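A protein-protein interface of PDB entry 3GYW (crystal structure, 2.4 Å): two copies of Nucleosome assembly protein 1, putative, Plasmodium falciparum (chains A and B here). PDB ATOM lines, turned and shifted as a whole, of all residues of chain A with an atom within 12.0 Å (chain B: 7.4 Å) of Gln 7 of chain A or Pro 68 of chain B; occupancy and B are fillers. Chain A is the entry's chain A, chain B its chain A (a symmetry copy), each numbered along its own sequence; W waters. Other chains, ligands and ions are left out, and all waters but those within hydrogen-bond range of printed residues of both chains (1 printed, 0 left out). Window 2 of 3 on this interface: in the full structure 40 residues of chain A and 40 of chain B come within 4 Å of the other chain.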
ATOM      1  N   LEU A   3     -20.374   4.937   1.678  1.00  0.00           N
ATOM      2  CA  LEU A   3     -20.232   4.507   0.256  1.00  0.00           C
ATOM      3  C   LEU A   3     -20.132   2.997   0.149  1.00  0.00           C
ATOM      4  O   LEU A   3     -19.533   2.344   1.007  1.00  0.00           O
ATOM      5  CB  LEU A   3     -18.981   5.123  -0.386  1.00  0.00           C
ATOM      6  CG  LEU A   3     -18.770   6.638  -0.480  1.00  0.00           C
ATOM      7  CD1 LEU A   3     -17.435   6.926  -1.148  1.00  0.00           C
ATOM      8  CD2 LEU A   3     -19.904   7.323  -1.230  1.00  0.00           C
ATOM      9  N   THR A   4     -20.701   2.446  -0.921  1.00  0.00           N
ATOM     10  CA  THR A   4     -20.533   1.033  -1.227  1.00  0.00           C
ATOM     11  C   THR A   4     -19.114   0.826  -1.761  1.00  0.00           C
ATOM     12  O   THR A   4     -18.415   1.803  -2.071  1.00  0.00           O
ATOM     13  CB  THR A   4     -21.566   0.533  -2.266  1.00  0.00           C
ATOM     14  OG1 THR A   4     -21.267   1.082  -3.558  1.00  0.00           O
ATOM     15  CG2 THR A   4     -23.002   0.904  -1.853  1.00  0.00           C
ATOM     16  N   GLU A   5     -18.693  -0.431  -1.873  1.00  0.00           N
ATOM     17  CA  GLU A   5     -17.347  -0.741  -2.346  1.00  0.00           C
ATOM     18  C   GLU A   5     -17.153  -0.375  -3.819  1.00  0.00           C
ATOM     19  O   GLU A   5     -16.070   0.047  -4.227  1.00  0.00           O
ATOM     20  CB  GLU A   5     -16.989  -2.215  -2.106  1.00  0.00           C
ATOM     21  CG  GLU A   5     -17.430  -2.809  -0.752  1.00  0.00           C
ATOM     22  CD  GLU A   5     -17.157  -1.929   0.446  1.00  0.00           C
ATOM     23  OE1 GLU A   5     -16.025  -1.423   0.575  1.00  0.00           O
ATOM     24  OE2 GLU A   5     -18.074  -1.754   1.269  1.00  0.00           O
ATOM     25  N   GLU A   6     -18.209  -0.535  -4.605  1.00  0.00           N
ATOM     26  CA  GLU A   6     -18.187  -0.159  -6.012  1.00  0.00           C
ATOM     27  C   GLU A   6     -17.970   1.351  -6.164  1.00  0.00           C
ATOM     28  O   GLU A   6     -17.218   1.794  -7.025  1.00  0.00           O
ATOM     29  CB  GLU A   6     -19.487  -0.589  -6.685  1.00  0.00           C
ATOM     30  CG  GLU A   6     -19.340  -0.979  -8.150  1.00  0.00           C
ATOM     31  CD  GLU A   6     -20.689  -1.229  -8.823  1.00  0.00           C
ATOM     32  OE1 GLU A   6     -20.820  -0.923 -10.029  1.00  0.00           O
ATOM     33  OE2 GLU A   6     -21.621  -1.725  -8.146  1.00  0.00           O
ATOM     34  N   GLN A   7     -18.621   2.125  -5.300  1.00  0.00           N
ATOM     35  CA  GLN A   7     -18.450   3.568  -5.257  1.00  0.00           C
ATOM     36  C   GLN A   7     -17.063   3.985  -4.749  1.00  0.00           C
ATOM     37  O   GLN A   7     -16.481   4.948  -5.252  1.00  0.00           O
ATOM     38  CB  GLN A   7     -19.572   4.202  -4.433  1.00  0.00           C
ATOM     39  CG  GLN A   7     -20.946   4.096  -5.108  1.00  0.00           C
ATOM     40  CD  GLN A   7     -22.122   4.248  -4.146  1.00  0.00           C
ATOM     41  OE1 GLN A   7     -21.946   4.548  -2.961  1.00  0.00           O
ATOM     42  NE2 GLN A   7     -23.334   4.038  -4.659  1.00  0.00           N
ATOM     43  N   LYS A   8     -16.533   3.244  -3.774  1.00  0.00           N
ATOM     44  CA  LYS A   8     -15.171   3.447  -3.278  1.00  0.00           C
ATOM     45  C   LYS A   8     -14.135   3.256  -4.385  1.00  0.00           C
ATOM     46  O   LYS A   8     -13.119   3.959  -4.419  1.00  0.00           O
ATOM     47  CB  LYS A   8     -14.858   2.496  -2.117  1.00  0.00           C
ATOM     48  CG  LYS A   8     -15.456   2.876  -0.767  1.00  0.00           C
ATOM     49  CD  LYS A   8     -15.125   1.806   0.276  1.00  0.00           C
ATOM     50  CE  LYS A   8     -16.178   1.709   1.381  1.00  0.00           C
ATOM     51  NZ  LYS A   8     -16.236   2.932   2.246  1.00  0.00           N
ATOM     52  N   GLU A   9     -14.397   2.299  -5.275  1.00  0.00           N
ATOM     53  CA  GLU A   9     -13.561   2.050  -6.449  1.00  0.00           C
ATOM     54  C   GLU A   9     -13.583   3.210  -7.445  1.00  0.00           C
ATOM     55  O   GLU A   9     -12.552   3.572  -8.006  1.00  0.00           O
ATOM     56  CB  GLU A   9     -14.001   0.766  -7.151  1.00  0.00           C
ATOM     57  CG  GLU A   9     -13.448  -0.505  -6.542  1.00  0.00           C
ATOM     58  CD  GLU A   9     -12.042  -0.845  -7.035  1.00  0.00           C
ATOM     59  OE1 GLU A   9     -11.737  -2.050  -7.148  1.00  0.00           O
ATOM     60  OE2 GLU A   9     -11.239   0.082  -7.307  1.00  0.00           O
ATOM     61  N   THR A  10     -14.766   3.779  -7.664  1.00  0.00           N
ATOM     62  CA  THR A  10     -14.922   4.952  -8.514  1.00  0.00           C
ATOM     63  C   THR A  10     -14.154   6.137  -7.929  1.00  0.00           C
ATOM     64  O   THR A  10     -13.419   6.824  -8.643  1.00  0.00           O
ATOM     65  CB  THR A  10     -16.410   5.305  -8.690  1.00  0.00           C
ATOM     66  OG1 THR A  10     -17.087   4.196  -9.297  1.00  0.00           O
ATOM     67  CG2 THR A  10     -16.585   6.554  -9.560  1.00  0.00           C
ATOM     68  N   LEU A  11     -14.316   6.351  -6.625  1.00  0.00           N
ATOM     69  CA  LEU A  11     -13.599   7.400  -5.896  1.00  0.00           C
ATOM     70  C   LEU A  11     -12.081   7.237  -6.022  1.00  0.00           C
ATOM     71  O   LEU A  11     -11.360   8.216  -6.239  1.00  0.00           O
ATOM     72  CB  LEU A  11     -14.018   7.393  -4.423  1.00  0.00           C
ATOM     73  CG  LEU A  11     -13.612   8.563  -3.529  1.00  0.00           C
ATOM     74  CD1 LEU A  11     -14.183   9.876  -4.041  1.00  0.00           C
ATOM     75  CD2 LEU A  11     -14.059   8.313  -2.099  1.00  0.00           C
ATOM     76  N   LYS A  12     -11.623   5.992  -5.891  1.00  0.00           N
ATOM     77  CA  LYS A  12     -10.219   5.624  -6.053  1.00  0.00           C
ATOM     78  C   LYS A  12      -9.690   6.078  -7.416  1.00  0.00           C
ATOM     79  O   LYS A  12      -8.661   6.748  -7.487  1.00  0.00           O
ATOM     80  CB  LYS A  12     -10.054   4.105  -5.857  1.00  0.00           C
ATOM     81  CG  LYS A  12      -8.793   3.486  -6.444  1.00  0.00           C
ATOM     82  CD  LYS A  12      -7.851   2.988  -5.372  1.00  0.00           C
ATOM     83  CE  LYS A  12      -6.665   2.236  -5.978  1.00  0.00           C
ATOM     84  NZ  LYS A  12      -7.046   0.872  -6.425  1.00  0.00           N
ATOM     85  N   LYS A  13     -10.402   5.716  -8.482  1.00  0.00           N
ATOM     86  CA  LYS A  13     -10.071   6.144  -9.849  1.00  0.00           C
ATOM     87  C   LYS A  13      -9.980   7.665  -9.989  1.00  0.00           C
ATOM     88  O   LYS A  13      -9.011   8.187 -10.546  1.00  0.00           O
ATOM     89  CB  LYS A  13     -11.104   5.600 -10.838  1.00  0.00           C
ATOM     90  CG  LYS A  13     -11.056   4.087 -11.028  1.00  0.00           C
ATOM     91  CD  LYS A  13     -12.036   3.655 -12.111  1.00  0.00           C
ATOM     92  CE  LYS A  13     -12.154   2.142 -12.202  1.00  0.00           C
ATOM     93  NZ  LYS A  13     -13.472   1.779 -12.829  1.00  0.00           N
ATOM     94  N   LEU A  14     -10.987   8.364  -9.467  1.00  0.00           N
ATOM     95  CA  LEU A  14     -11.040   9.823  -9.495  1.00  0.00           C
ATOM     96  C   LEU A  14      -9.882  10.491  -8.747  1.00  0.00           C
ATOM     97  O   LEU A  14      -9.408  11.542  -9.161  1.00  0.00           O
ATOM     98  CB  LEU A  14     -12.386  10.323  -8.962  1.00  0.00           C
ATOM     99  CG  LEU A  14     -13.517  10.547  -9.974  1.00  0.00           C
ATOM    100  CD1 LEU A  14     -13.886   9.287 -10.742  1.00  0.00           C
ATOM    101  CD2 LEU A  14     -14.746  11.120  -9.284  1.00  0.00           C
ATOM    102  N   LYS A  15      -9.430   9.875  -7.655  1.00  0.00           N
ATOM    103  CA  LYS A  15      -8.252  10.358  -6.923  1.00  0.00           C
ATOM    104  C   LYS A  15      -7.000  10.209  -7.776  1.00  0.00           C
ATOM    105  O   LYS A  15      -6.171  11.110  -7.816  1.00  0.00           O
ATOM    106  CB  LYS A  15      -8.074   9.611  -5.599  1.00  0.00           C
ATOM    107  CG  LYS A  15      -9.019  10.044  -4.496  1.00  0.00           C
ATOM    108  CD  LYS A  15      -9.029   9.031  -3.356  1.00  0.00           C
ATOM    109  CE  LYS A  15      -9.540   9.657  -2.072  1.00  0.00           C
ATOM    110  NZ  LYS A  15      -9.888   8.632  -1.048  1.00  0.00           N
ATOM    111  N   LEU A  16      -6.881   9.072  -8.458  1.00  0.00           N
ATOM    112  CA  LEU A  16      -5.789   8.826  -9.400  1.00  0.00           C
ATOM    113  C   LEU A  16      -5.766   9.872 -10.521  1.00  0.00           C
ATOM    114  O   LEU A  16      -4.719  10.442 -10.805  1.00  0.00           O
ATOM    115  CB  LEU A  16      -5.870   7.403  -9.987  1.00  0.00           C
ATOM    116  CG  LEU A  16      -4.894   7.026 -11.121  1.00  0.00           C
ATOM    117  CD1 LEU A  16      -3.514   6.633 -10.584  1.00  0.00           C
ATOM    118  CD2 LEU A  16      -5.451   5.911 -12.008  1.00  0.00           C
ATOM    119  N   TYR A  17      -6.920  10.116 -11.142  1.00  0.00           N
ATOM    120  CA  TYR A  17      -7.014  11.085 -12.231  1.00  0.00           C
ATOM    121  C   TYR A  17      -6.749  12.519 -11.771  1.00  0.00           C
ATOM    122  O   TYR A  17      -6.196  13.312 -12.523  1.00  0.00           O
ATOM    123  CB  TYR A  17      -8.376  11.025 -12.936  1.00  0.00           C
ATOM    124  CG  TYR A  17      -8.850   9.650 -13.363  1.00  0.00           C
ATOM    125  CD1 TYR A  17      -7.955   8.679 -13.825  1.00  0.00           C
ATOM    126  CD2 TYR A  17     -10.209   9.336 -13.344  1.00  0.00           C
ATOM    127  CE1 TYR A  17      -8.399   7.426 -14.227  1.00  0.00           C
ATOM    128  CE2 TYR A  17     -10.664   8.087 -13.747  1.00  0.00           C
ATOM    129  CZ  TYR A  17      -9.752   7.137 -14.185  1.00  0.00           C
ATOM    130  OH  TYR A  17     -10.202   5.900 -14.588  1.00  0.00           O
ATOM    131  N   LEU B  54     -17.497   7.879 -13.571  1.00  0.00           N
ATOM    132  CA  LEU B  54     -18.677   8.361 -12.854  1.00  0.00           C
ATOM    133  C   LEU B  54     -19.984   7.832 -13.439  1.00  0.00           C
ATOM    134  O   LEU B  54     -20.895   7.443 -12.705  1.00  0.00           O
ATOM    135  CB  LEU B  54     -18.711   9.894 -12.864  1.00  0.00           C
ATOM    136  CG  LEU B  54     -17.790  10.672 -11.927  1.00  0.00           C
ATOM    137  CD1 LEU B  54     -17.853  12.143 -12.261  1.00  0.00           C
ATOM    138  CD2 LEU B  54     -18.138  10.435 -10.470  1.00  0.00           C
ATOM    139  N   ILE B  62     -30.236   8.267 -13.463  1.00  0.00           N
ATOM    140  CA  ILE B  62     -29.748   9.153 -12.409  1.00  0.00           C
ATOM    141  C   ILE B  62     -28.349   9.638 -12.809  1.00  0.00           C
ATOM    142  O   ILE B  62     -27.670   8.993 -13.608  1.00  0.00           O
ATOM    143  CB  ILE B  62     -29.764   8.459 -11.008  1.00  0.00           C
ATOM    144  CG1 ILE B  62     -29.714   9.485  -9.864  1.00  0.00           C
ATOM    145  CG2 ILE B  62     -28.636   7.427 -10.869  1.00  0.00           C
ATOM    146  CD1 ILE B  62     -30.957  10.366  -9.726  1.00  0.00           C
ATOM    147  N   GLY B  63     -27.931  10.782 -12.279  1.00  0.00           N
ATOM    148  CA  GLY B  63     -26.626  11.349 -12.611  1.00  0.00           C
ATOM    149  C   GLY B  63     -25.491  10.658 -11.891  1.00  0.00           C
ATOM    150  O   GLY B  63     -25.648  10.218 -10.753  1.00  0.00           O
ATOM    151  N   THR B  64     -24.342  10.579 -12.562  1.00  0.00           N
ATOM    152  CA  THR B  64     -23.148   9.883 -12.056  1.00  0.00           C
ATOM    153  C   THR B  64     -23.486   8.642 -11.215  1.00  0.00           C
ATOM    154  O   THR B  64     -23.173   8.597 -10.024  1.00  0.00           O
ATOM    155  CB  THR B  64     -22.226  10.827 -11.252  1.00  0.00           C
ATOM    156  OG1 THR B  64     -22.961  11.399 -10.166  1.00  0.00           O
ATOM    157  CG2 THR B  64     -21.682  11.937 -12.135  1.00  0.00           C
ATOM    158  N   PRO B  65     -24.125   7.628 -11.839  1.00  0.00           N
ATOM    159  CA  PRO B  65     -24.629   6.481 -11.072  1.00  0.00           C
ATOM    160  C   PRO B  65     -23.548   5.646 -10.377  1.00  0.00           C
ATOM    161  O   PRO B  65     -23.855   4.937  -9.417  1.00  0.00           O
ATOM    162  CB  PRO B  65     -25.384   5.650 -12.117  1.00  0.00           C
ATOM    163  CG  PRO B  65     -24.833   6.085 -13.432  1.00  0.00           C
ATOM    164  CD  PRO B  65     -24.414   7.504 -13.281  1.00  0.00           C
ATOM    165  N   ASN B  66     -22.301   5.739 -10.839  1.00  0.00           N
ATOM    166  CA  ASN B  66     -21.190   5.058 -10.166  1.00  0.00           C
ATOM    167  C   ASN B  66     -20.724   5.754  -8.891  1.00  0.00           C
ATOM    168  O   ASN B  66     -20.004   5.160  -8.086  1.00  0.00           O
ATOM    169  CB  ASN B  66     -20.010   4.854 -11.117  1.00  0.00           C
ATOM    170  CG  ASN B  66     -20.320   3.878 -12.241  1.00  0.00           C
ATOM    171  OD1 ASN B  66     -21.161   2.984 -12.096  1.00  0.00           O
ATOM    172  ND2 ASN B  66     -19.636   4.041 -13.367  1.00  0.00           N
ATOM    173  N   LEU B  67     -21.123   7.013  -8.720  1.00  0.00           N
ATOM    174  CA  LEU B  67     -20.846   7.773  -7.497  1.00  0.00           C
ATOM    175  C   LEU B  67     -21.923   8.850  -7.292  1.00  0.00           C
ATOM    176  O   LEU B  67     -21.734  10.005  -7.669  1.00  0.00           O
ATOM    177  CB  LEU B  67     -19.439   8.386  -7.537  1.00  0.00           C
ATOM    178  CG  LEU B  67     -18.822   8.956  -6.254  1.00  0.00           C
ATOM    179  CD1 LEU B  67     -18.706   7.885  -5.173  1.00  0.00           C
ATOM    180  CD2 LEU B  67     -17.458   9.550  -6.562  1.00  0.00           C
ATOM    181  N   PRO B  68     -23.060   8.466  -6.685  1.00  0.00           N
ATOM    182  CA  PRO B  68     -24.253   9.310  -6.599  1.00  0.00           C
ATOM    183  C   PRO B  68     -23.978  10.705  -6.053  1.00  0.00           C
ATOM    184  O   PRO B  68     -23.166  10.862  -5.137  1.00  0.00           O
ATOM    185  CB  PRO B  68     -25.153   8.534  -5.630  1.00  0.00           C
ATOM    186  CG  PRO B  68     -24.759   7.121  -5.824  1.00  0.00           C
ATOM    187  CD  PRO B  68     -23.268   7.163  -6.021  1.00  0.00           C
ATOM    188  N   GLU B  69     -24.657  11.698  -6.634  1.00  0.00           N
ATOM    189  CA  GLU B  69     -24.604  13.106  -6.204  1.00  0.00           C
ATOM    190  C   GLU B  69     -23.205  13.736  -6.266  1.00  0.00           C
ATOM    191  O   GLU B  69     -22.903  14.661  -5.500  1.00  0.00           O
ATOM    192  CB  GLU B  69     -25.187  13.279  -4.790  1.00  0.00           C
ATOM    193  CG  GLU B  69     -26.440  12.459  -4.492  1.00  0.00           C
ATOM    194  CD  GLU B  69     -27.040  12.774  -3.127  1.00  0.00           C
ATOM    195  OE1 GLU B  69     -26.293  13.163  -2.195  1.00  0.00           O
ATOM    196  OE2 GLU B  69     -28.272  12.639  -2.988  1.00  0.00           O
ATOM    197  N   PHE B  70     -22.355  13.246  -7.166  1.00  0.00           N
ATOM    198  CA  PHE B  70     -20.962  13.697  -7.213  1.00  0.00           C
ATOM    199  C   PHE B  70     -20.808  15.203  -7.447  1.00  0.00           C
ATOM    200  O   PHE B  70     -20.026  15.862  -6.769  1.00  0.00           O
ATOM    201  CB  PHE B  70     -20.143  12.931  -8.267  1.00  0.00           C
ATOM    202  CG  PHE B  70     -18.746  13.479  -8.454  1.00  0.00           C
ATOM    203  CD1 PHE B  70     -17.745  13.203  -7.523  1.00  0.00           C
ATOM    204  CD2 PHE B  70     -18.444  14.301  -9.534  1.00  0.00           C
ATOM    205  CE1 PHE B  70     -16.464  13.719  -7.680  1.00  0.00           C
ATOM    206  CE2 PHE B  70     -17.166  14.815  -9.702  1.00  0.00           C
ATOM    207  CZ  PHE B  70     -16.174  14.526  -8.768  1.00  0.00           C
ATOM    208  N   TRP B  71     -21.522  15.727  -8.439  1.00  0.00           N
ATOM    209  CA  TRP B  71     -21.321  17.108  -8.871  1.00  0.00           C
ATOM    210  C   TRP B  71     -22.032  18.082  -7.938  1.00  0.00           C
ATOM    211  O   TRP B  71     -21.500  19.151  -7.633  1.00  0.00           O
ATOM    212  CB  TRP B  71     -21.753  17.302 -10.329  1.00  0.00           C
ATOM    213  CG  TRP B  71     -20.873  16.602 -11.330  1.00  0.00           C
ATOM    214  CD1 TRP B  71     -21.155  15.452 -12.007  1.00  0.00           C
ATOM    215  CD2 TRP B  71     -19.573  17.017 -11.778  1.00  0.00           C
ATOM    216  NE1 TRP B  71     -20.113  15.116 -12.842  1.00  0.00           N
ATOM    217  CE2 TRP B  71     -19.131  16.063 -12.725  1.00  0.00           C
ATOM    218  CE3 TRP B  71     -18.739  18.106 -11.478  1.00  0.00           C
ATOM    219  CZ2 TRP B  71     -17.895  16.161 -13.367  1.00  0.00           C
ATOM    220  CZ3 TRP B  71     -17.512  18.205 -12.122  1.00  0.00           C
ATOM    221  CH2 TRP B  71     -17.101  17.236 -13.052  1.00  0.00           C
ATOM    222  N   LEU B  72     -23.220  17.694  -7.474  1.00  0.00           N
ATOM    223  CA  LEU B  72     -23.935  18.438  -6.440  1.00  0.00           C
ATOM    224  C   LEU B  72     -23.050  18.715  -5.224  1.00  0.00           C
ATOM    225  O   LEU B  72     -22.948  19.857  -4.786  1.00  0.00           O
ATOM    226  CB  LEU B  72     -25.217  17.705  -6.007  1.00  0.00           C
ATOM    227  CG  LEU B  72     -26.020  18.293  -4.828  1.00  0.00           C
ATOM    228  CD1 LEU B  72     -26.408  19.764  -5.031  1.00  0.00           C
ATOM    229  CD2 LEU B  72     -27.247  17.457  -4.537  1.00  0.00           C
ATOM    230  N   ARG B  73     -22.417  17.671  -4.692  1.00  0.00           N
ATOM    231  CA  ARG B  73     -21.568  17.804  -3.504  1.00  0.00           C
ATOM    232  C   ARG B  73     -20.284  18.593  -3.761  1.00  0.00           C
ATOM    233  O   ARG B  73     -19.823  19.324  -2.888  1.00  0.00           O
ATOM    234  CB  ARG B  73     -21.262  16.434  -2.904  1.00  0.00           C
ATOM    235  CG  ARG B  73     -22.496  15.749  -2.352  1.00  0.00           C
ATOM    236  CD  ARG B  73     -22.218  14.334  -1.884  1.00  0.00           C
ATOM    237  NE  ARG B  73     -23.443  13.742  -1.343  1.00  0.00           N
ATOM    238  CZ  ARG B  73     -23.535  12.518  -0.826  1.00  0.00           C
ATOM    239  NH1 ARG B  73     -22.470  11.719  -0.777  1.00  0.00           N
ATOM    240  NH2 ARG B  73     -24.704  12.092  -0.357  1.00  0.00           N
ATOM    241  N   VAL B  94     -28.749  16.312  -8.845  1.00  0.00           N
ATOM    242  CA  VAL B  94     -28.414  14.891  -8.714  1.00  0.00           C
ATOM    243  C   VAL B  94     -28.389  14.138 -10.067  1.00  0.00           C
ATOM    244  O   VAL B  94     -27.765  13.077 -10.186  1.00  0.00           O
ATOM    245  CB  VAL B  94     -29.332  14.179  -7.687  1.00  0.00           C
ATOM    246  CG1 VAL B  94     -28.970  14.615  -6.283  1.00  0.00           C
ATOM    247  CG2 VAL B  94     -30.809  14.462  -7.969  1.00  0.00           C
ATOM    248  N   TYR B 245     -15.616  17.553  -3.880  1.00  0.00           N
ATOM    249  CA  TYR B 245     -16.451  16.429  -3.439  1.00  0.00           C
ATOM    250  C   TYR B 245     -16.026  15.896  -2.067  1.00  0.00           C
ATOM    251  O   TYR B 245     -16.869  15.664  -1.199  1.00  0.00           O
ATOM    252  CB  TYR B 245     -16.447  15.290  -4.468  1.00  0.00           C
ATOM    253  CG  TYR B 245     -17.141  14.035  -3.977  1.00  0.00           C
ATOM    254  CD1 TYR B 245     -18.516  13.857  -4.154  1.00  0.00           C
ATOM    255  CD2 TYR B 245     -16.423  13.031  -3.318  1.00  0.00           C
ATOM    256  CE1 TYR B 245     -19.156  12.705  -3.696  1.00  0.00           C
ATOM    257  CE2 TYR B 245     -17.050  11.881  -2.850  1.00  0.00           C
ATOM    258  CZ  TYR B 245     -18.416  11.723  -3.041  1.00  0.00           C
ATOM    259  OH  TYR B 245     -19.033  10.580  -2.580  1.00  0.00           O
HETATM  260  O   HOH W   1     -20.573   2.423  -8.041  1.00  0.00           O
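Printed residues of chain B that touch a printed residue of chain A: Leu 54, Asn 66, Leu 67, Pro 68, Phe 70 and Tyr 245.
Hydrophobic or aromatic side chains of chain B that line the printed part of chain A: Leu 54, Leu 67, Pro 68, Phe 70 and Tyr 245.
Among the printed residues, 9 pairs touch across the chains.
Water W1 lies within hydrogen-bond range of O of Asn 66 of chain B (2.8 Å) and N of Gln 7 of chain A (3.4 Å).
No position is printed for both chains.
Of the 9 pairs that touch across the chains among the printed residues, none has its exchanged pair printed and touching as well.
Leu 3 of chain A touches Tyr 245 of chain B (CD2 to OH, 3.6 Å).
Gln 7 of chain A touches Asn 66 of chain B.
Leu 67 of chain B touches Gln 7 of chain A (CD1 to O, 3.7 Å).
NE2 of Gln 7 of chain A touches CD of Pro 68 of chain B, at 3.4 Å.
Thr 10 of chain A touches Leu 67 of chain B.
Leu 11 of chain A touches Tyr 245 of chain B.
Leu 14 of chain A touches Leu 54 of chain B (CD2 to CD2, 3.7 Å).
CE1 of Phe 70 of chain B touches CD2 of Leu 14 of chain A, 3.5 Å away.
The backbone NH (N) of Thr 4 of chain A lies within hydrogen-bond range of the side-chain amide oxygen (OE1) of Gln 7 of chain A (3.2 Å).
The backbone carbonyl oxygen of Glu 6 of chain A is in hydrogen-bond range of the side-chain hydroxyl of Thr 10 of chain A (3.3 Å).
O of Leu 54 of chain B sits at hydrogen-bond distance from N of Asn 66 of chain B (2.9 Å).
OG1 of Thr 64 of chain B lies within hydrogen-bond range of O of Leu 67 of chain B, 3.1 Å away.
The side-chain hydroxyl (OG1) of Thr 10 of chain A is in hydrogen-bond range of the backbone carbonyl oxygen (O) of Asn 66 of chain B, 3.3 Å away.
Of chain B, only Asn 66 (3.3 Å), Leu 67 (3.7 Å) and Pro 68 (3.4 Å) come within 4 Å of Gln 7 of chain A.
Of chain A, only Gln 7 comes within 4 Å of Pro 68 of chain B.
Leu 67 of chain B touches just these residues of chain A: Gln 7 and Thr 10.
No residue of chain A comes within 4 Å of Glu 69 of chain B.
Printed residues of chain B within 4 Å of Leu 14 of chain A: Leu 54 (3.7 Å) and Phe 70 (3.5 Å).
Of the printed residues of chain A, Asn 66 of chain B touches Gln 7 and Thr 10.
Of the printed residues of chain A, Tyr 245 of chain B touches Leu 3 and Leu 11.
Glu 5 of chain A touches none of the printed residues of chain B.
Lys 15 of chain A touches none of the printed residues of chain B.
The nearest residue of chain B that does not touch Gln 7 of chain A is Pro 65 of chain B (4.9 Å).
The nearest residue of chain A that does not touch Pro 68 of chain B is Leu 3 of chain A (5.9 Å).
The nearest printed residue of chain A that does not touch Asn 66 of chain B is Glu 6 of chain A (4.4 Å).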
